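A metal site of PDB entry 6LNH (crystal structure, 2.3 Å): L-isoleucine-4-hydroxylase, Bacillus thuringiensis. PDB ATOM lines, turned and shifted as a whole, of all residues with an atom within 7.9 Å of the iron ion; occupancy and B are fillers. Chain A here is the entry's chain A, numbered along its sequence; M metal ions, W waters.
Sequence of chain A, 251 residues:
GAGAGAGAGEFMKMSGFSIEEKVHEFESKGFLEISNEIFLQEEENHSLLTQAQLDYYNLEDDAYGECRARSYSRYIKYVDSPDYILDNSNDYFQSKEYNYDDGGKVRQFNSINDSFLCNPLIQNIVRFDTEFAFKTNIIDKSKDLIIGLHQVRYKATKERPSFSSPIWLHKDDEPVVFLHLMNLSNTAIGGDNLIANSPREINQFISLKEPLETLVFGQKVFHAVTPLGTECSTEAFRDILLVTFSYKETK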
ATOM      1  N   TYR A 154       3.498   6.407 -12.895  1.00  0.00           N
ATOM      2  CA  TYR A 154       2.121   6.873 -13.026  1.00  0.00           C
ATOM      3  C   TYR A 154       2.124   8.372 -13.173  1.00  0.00           C
ATOM      4  O   TYR A 154       2.898   9.066 -12.501  1.00  0.00           O
ATOM      5  CB  TYR A 154       1.249   6.474 -11.836  1.00  0.00           C
ATOM      6  CG  TYR A 154       1.137   5.010 -11.634  1.00  0.00           C
ATOM      7  CD1 TYR A 154       2.174   4.292 -11.069  1.00  0.00           C
ATOM      8  CD2 TYR A 154       0.004   4.321 -12.050  1.00  0.00           C
ATOM      9  CE1 TYR A 154       2.081   2.953 -10.898  1.00  0.00           C
ATOM     10  CE2 TYR A 154      -0.104   2.968 -11.872  1.00  0.00           C
ATOM     11  CZ  TYR A 154       0.949   2.291 -11.299  1.00  0.00           C
ATOM     12  OH  TYR A 154       0.882   0.933 -11.108  1.00  0.00           O
ATOM     13  N   SER A 164      -4.431   2.135 -12.083  1.00  0.00           N
ATOM     14  CA  SER A 164      -3.716   0.900 -12.368  1.00  0.00           C
ATOM     15  C   SER A 164      -4.580  -0.009 -13.234  1.00  0.00           C
ATOM     16  O   SER A 164      -5.756   0.251 -13.465  1.00  0.00           O
ATOM     17  CB  SER A 164      -3.340   0.191 -11.070  1.00  0.00           C
ATOM     18  OG  SER A 164      -2.137  -0.557 -11.222  1.00  0.00           O
ATOM     19  N   SER A 165      -3.976  -1.091 -13.723  1.00  0.00           N
ATOM     20  CA  SER A 165      -4.729  -2.152 -14.396  1.00  0.00           C
ATOM     21  C   SER A 165      -4.342  -3.468 -13.773  1.00  0.00           C
ATOM     22  O   SER A 165      -3.169  -3.874 -13.859  1.00  0.00           O
ATOM     23  CB  SER A 165      -4.441  -2.142 -15.898  1.00  0.00           C
ATOM     24  OG  SER A 165      -4.499  -3.454 -16.431  1.00  0.00           O
ATOM     25  N   PRO A 166      -5.288  -4.207 -13.139  1.00  0.00           N
ATOM     26  CA  PRO A 166      -6.712  -3.964 -12.871  1.00  0.00           C
ATOM     27  C   PRO A 166      -7.006  -2.696 -12.047  1.00  0.00           C
ATOM     28  O   PRO A 166      -6.145  -2.193 -11.332  1.00  0.00           O
ATOM     29  CB  PRO A 166      -7.141  -5.204 -12.081  1.00  0.00           C
ATOM     30  CG  PRO A 166      -6.103  -6.222 -12.372  1.00  0.00           C
ATOM     31  CD  PRO A 166      -4.833  -5.452 -12.499  1.00  0.00           C
ATOM     32  N   TRP A 168      -9.323  -2.243  -9.587  1.00  0.00           N
ATOM     33  CA  TRP A 168      -9.775  -2.417  -8.208  1.00  0.00           C
ATOM     34  C   TRP A 168      -9.051  -3.636  -7.617  1.00  0.00           C
ATOM     35  O   TRP A 168      -7.969  -4.023  -8.065  1.00  0.00           O
ATOM     36  CB  TRP A 168     -11.316  -2.515  -8.195  1.00  0.00           C
ATOM     37  CG  TRP A 168     -11.968  -2.623  -6.838  1.00  0.00           C
ATOM     38  CD1 TRP A 168     -12.910  -3.545  -6.463  1.00  0.00           C
ATOM     39  CD2 TRP A 168     -11.737  -1.803  -5.687  1.00  0.00           C
ATOM     40  NE1 TRP A 168     -13.276  -3.348  -5.163  1.00  0.00           N
ATOM     41  CE2 TRP A 168     -12.571  -2.280  -4.657  1.00  0.00           C
ATOM     42  CE3 TRP A 168     -10.907  -0.707  -5.418  1.00  0.00           C
ATOM     43  CZ2 TRP A 168     -12.607  -1.713  -3.379  1.00  0.00           C
ATOM     44  CZ3 TRP A 168     -10.942  -0.138  -4.150  1.00  0.00           C
ATOM     45  CH2 TRP A 168     -11.790  -0.639  -3.145  1.00  0.00           C
ATOM     46  N   HIS A 170      -7.660  -7.204  -6.605  1.00  0.00           N
ATOM     47  CA  HIS A 170      -7.232  -8.244  -7.524  1.00  0.00           C
ATOM     48  C   HIS A 170      -6.071  -9.004  -6.880  1.00  0.00           C
ATOM     49  O   HIS A 170      -5.566  -8.630  -5.826  1.00  0.00           O
ATOM     50  CB  HIS A 170      -6.802  -7.666  -8.867  1.00  0.00           C
ATOM     51  CG  HIS A 170      -5.568  -6.818  -8.783  1.00  0.00           C
ATOM     52  ND1 HIS A 170      -5.589  -5.502  -8.381  1.00  0.00           N
ATOM     53  CD2 HIS A 170      -4.268  -7.103  -9.051  1.00  0.00           C
ATOM     54  CE1 HIS A 170      -4.359  -5.010  -8.400  1.00  0.00           C
ATOM     55  NE2 HIS A 170      -3.540  -5.962  -8.797  1.00  0.00           N
ATOM     56  N   LYS A 171      -5.678 -10.088  -7.544  1.00  0.00           N
ATOM     57  CA  LYS A 171      -4.462 -10.809  -7.224  1.00  0.00           C
ATOM     58  C   LYS A 171      -3.576 -10.848  -8.466  1.00  0.00           C
ATOM     59  O   LYS A 171      -4.071 -10.997  -9.587  1.00  0.00           O
ATOM     60  CB  LYS A 171      -4.748 -12.228  -6.730  1.00  0.00           C
ATOM     61  CG  LYS A 171      -5.490 -12.253  -5.410  1.00  0.00           C
ATOM     62  CD  LYS A 171      -5.607 -13.659  -4.886  1.00  0.00           C
ATOM     63  CE  LYS A 171      -6.579 -13.718  -3.719  1.00  0.00           C
ATOM     64  NZ  LYS A 171      -6.763 -15.114  -3.230  1.00  0.00           N
ATOM     65  N   ASP A 172      -2.273 -10.704  -8.264  1.00  0.00           N
ATOM     66  CA  ASP A 172      -1.370 -10.746  -9.393  1.00  0.00           C
ATOM     67  C   ASP A 172      -1.061 -12.197  -9.784  1.00  0.00           C
ATOM     68  O   ASP A 172      -1.196 -13.128  -8.979  1.00  0.00           O
ATOM     69  CB  ASP A 172      -0.093  -9.966  -9.071  1.00  0.00           C
ATOM     70  CG  ASP A 172      -0.379  -8.488  -8.825  1.00  0.00           C
ATOM     71  OD1 ASP A 172      -1.483  -8.037  -9.203  1.00  0.00           O
ATOM     72  OD2 ASP A 172       0.478  -7.768  -8.262  1.00  0.00           O
ATOM     73  N   ASP A 173      -0.655 -12.376 -11.037  1.00  0.00           N
ATOM     74  CA  ASP A 173      -0.367 -13.705 -11.555  1.00  0.00           C
ATOM     75  C   ASP A 173       0.809 -14.363 -10.834  1.00  0.00           C
ATOM     76  O   ASP A 173       0.843 -15.589 -10.704  1.00  0.00           O
ATOM     77  CB  ASP A 173      -0.111 -13.643 -13.053  1.00  0.00           C
ATOM     78  CG  ASP A 173      -1.371 -13.309 -13.831  1.00  0.00           C
ATOM     79  OD1 ASP A 173      -2.457 -13.786 -13.448  1.00  0.00           O
ATOM     80  OD2 ASP A 173      -1.281 -12.553 -14.829  1.00  0.00           O
ATOM     81  N   GLU A 174       1.769 -13.561 -10.380  1.00  0.00           N
ATOM     82  CA  GLU A 174       2.986 -14.097  -9.768  1.00  0.00           C
ATOM     83  C   GLU A 174       2.769 -14.311  -8.278  1.00  0.00           C
ATOM     84  O   GLU A 174       2.200 -13.461  -7.596  1.00  0.00           O
ATOM     85  CB  GLU A 174       4.150 -13.135  -9.981  1.00  0.00           C
ATOM     86  CG  GLU A 174       4.379 -12.740 -11.443  1.00  0.00           C
ATOM     87  CD  GLU A 174       3.500 -11.585 -11.888  1.00  0.00           C
ATOM     88  OE1 GLU A 174       2.631 -11.149 -11.095  1.00  0.00           O
ATOM     89  OE2 GLU A 174       3.675 -11.106 -13.029  1.00  0.00           O
ATOM     90  N   VAL A 177       5.274 -10.853  -5.066  1.00  0.00           N
ATOM     91  CA  VAL A 177       5.496  -9.574  -5.740  1.00  0.00           C
ATOM     92  C   VAL A 177       6.011  -8.565  -4.725  1.00  0.00           C
ATOM     93  O   VAL A 177       5.434  -8.422  -3.638  1.00  0.00           O
ATOM     94  CB  VAL A 177       4.218  -9.061  -6.413  1.00  0.00           C
ATOM     95  CG1 VAL A 177       4.423  -7.683  -6.982  1.00  0.00           C
ATOM     96  CG2 VAL A 177       3.771 -10.020  -7.505  1.00  0.00           C
ATOM     97  N   LEU A 179       6.663  -4.555  -4.172  1.00  0.00           N
ATOM     98  CA  LEU A 179       6.378  -3.199  -4.625  1.00  0.00           C
ATOM     99  C   LEU A 179       7.303  -2.230  -3.897  1.00  0.00           C
ATOM    100  O   LEU A 179       7.211  -2.080  -2.676  1.00  0.00           O
ATOM    101  CB  LEU A 179       4.909  -2.833  -4.394  1.00  0.00           C
ATOM    102  CG  LEU A 179       4.539  -1.355  -4.534  1.00  0.00           C
ATOM    103  CD1 LEU A 179       5.009  -0.797  -5.855  1.00  0.00           C
ATOM    104  CD2 LEU A 179       3.036  -1.175  -4.385  1.00  0.00           C
ATOM    105  N   ASN A 193      -2.338   1.939  -0.951  1.00  0.00           N
ATOM    106  CA  ASN A 193      -2.434   0.494  -1.121  1.00  0.00           C
ATOM    107  C   ASN A 193      -3.462  -0.095  -0.169  1.00  0.00           C
ATOM    108  O   ASN A 193      -3.506   0.258   1.016  1.00  0.00           O
ATOM    109  CB  ASN A 193      -1.075  -0.176  -0.910  1.00  0.00           C
ATOM    110  CG  ASN A 193      -0.149   0.016  -2.084  1.00  0.00           C
ATOM    111  OD1 ASN A 193      -0.403  -0.482  -3.179  1.00  0.00           O
ATOM    112  ND2 ASN A 193       0.935   0.753  -1.870  1.00  0.00           N
ATOM    113  N   PHE A 217       3.511  -8.741  -1.686  1.00  0.00           N
ATOM    114  CA  PHE A 217       2.174  -9.318  -1.812  1.00  0.00           C
ATOM    115  C   PHE A 217       2.251 -10.820  -2.053  1.00  0.00           C
ATOM    116  O   PHE A 217       3.049 -11.289  -2.879  1.00  0.00           O
ATOM    117  CB  PHE A 217       1.379  -8.678  -2.952  1.00  0.00           C
ATOM    118  CG  PHE A 217       1.135  -7.213  -2.775  1.00  0.00           C
ATOM    119  CD1 PHE A 217       0.299  -6.745  -1.781  1.00  0.00           C
ATOM    120  CD2 PHE A 217       1.723  -6.295  -3.635  1.00  0.00           C
ATOM    121  CE1 PHE A 217       0.062  -5.392  -1.629  1.00  0.00           C
ATOM    122  CE2 PHE A 217       1.488  -4.940  -3.494  1.00  0.00           C
ATOM    123  CZ  PHE A 217       0.650  -4.488  -2.491  1.00  0.00           C
ATOM    124  N   HIS A 223      -5.311  -7.200  -3.232  1.00  0.00           N
ATOM    125  CA  HIS A 223      -4.775  -5.863  -3.061  1.00  0.00           C
ATOM    126  C   HIS A 223      -5.245  -4.966  -4.190  1.00  0.00           C
ATOM    127  O   HIS A 223      -5.796  -5.422  -5.200  1.00  0.00           O
ATOM    128  CB  HIS A 223      -3.244  -5.872  -2.979  1.00  0.00           C
ATOM    129  CG  HIS A 223      -2.572  -6.241  -4.272  1.00  0.00           C
ATOM    130  ND1 HIS A 223      -2.125  -7.511  -4.541  1.00  0.00           N
ATOM    131  CD2 HIS A 223      -2.266  -5.492  -5.360  1.00  0.00           C
ATOM    132  CE1 HIS A 223      -1.583  -7.533  -5.746  1.00  0.00           C
ATOM    133  NE2 HIS A 223      -1.653  -6.319  -6.258  1.00  0.00           N
ATOM    134  N   ALA A 224      -5.040  -3.668  -4.000  1.00  0.00           N
ATOM    135  CA  ALA A 224      -5.314  -2.645  -4.998  1.00  0.00           C
ATOM    136  C   ALA A 224      -4.497  -1.418  -4.640  1.00  0.00           C
ATOM    137  O   ALA A 224      -3.981  -1.291  -3.529  1.00  0.00           O
ATOM    138  CB  ALA A 224      -6.805  -2.323  -5.081  1.00  0.00           C
ATOM    139  N   VAL A 225      -4.348  -0.520  -5.611  1.00  0.00           N
ATOM    140  CA  VAL A 225      -3.811   0.814  -5.369  1.00  0.00           C
ATOM    141  C   VAL A 225      -4.832   1.821  -5.861  1.00  0.00           C
ATOM    142  O   VAL A 225      -5.244   1.774  -7.029  1.00  0.00           O
ATOM    143  CB  VAL A 225      -2.428   1.019  -6.024  1.00  0.00           C
ATOM    144  CG1 VAL A 225      -2.435   0.597  -7.478  1.00  0.00           C
ATOM    145  CG2 VAL A 225      -1.974   2.471  -5.865  1.00  0.00           C
ATOM    146  N   LEU A 242       8.514  -2.850  -9.446  1.00  0.00           N
ATOM    147  CA  LEU A 242       7.964  -4.135  -9.063  1.00  0.00           C
ATOM    148  C   LEU A 242       8.954  -5.248  -9.372  1.00  0.00           C
ATOM    149  O   LEU A 242       9.533  -5.297 -10.466  1.00  0.00           O
ATOM    150  CB  LEU A 242       6.637  -4.407  -9.784  1.00  0.00           C
ATOM    151  CG  LEU A 242       5.436  -3.653  -9.203  1.00  0.00           C
ATOM    152  CD1 LEU A 242       4.413  -3.295 -10.277  1.00  0.00           C
ATOM    153  CD2 LEU A 242       4.803  -4.437  -8.074  1.00  0.00           C
HETATM  154 FE    FE M   1      -1.034  -5.959  -8.405  1.00  0.00          FE
HETATM  155  O   HOH W   1      -0.530  -4.631 -10.129  1.00  0.00           O
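The iron ion is bound by water W1 (2.2 Å), a ring nitrogen (NE2) of His 223 (2.3 Å), the side-chain carboxylate (OD1) of Asp 172 (2.3 Å), the side-chain carboxylate (OD2) of Asp 172 (2.4 Å) and a ring nitrogen (NE2) of His 170 (2.5 Å).
Three residues have an atom within 4 Å of the iron ion: His 170, Asp 172 and His 223. The nearest printed residue that does not touch the iron ion is Lys 171 (5.5 Å).
O of Trp 168 lies within hydrogen-bond range of ND1 of His 170, at 2.8 Å.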
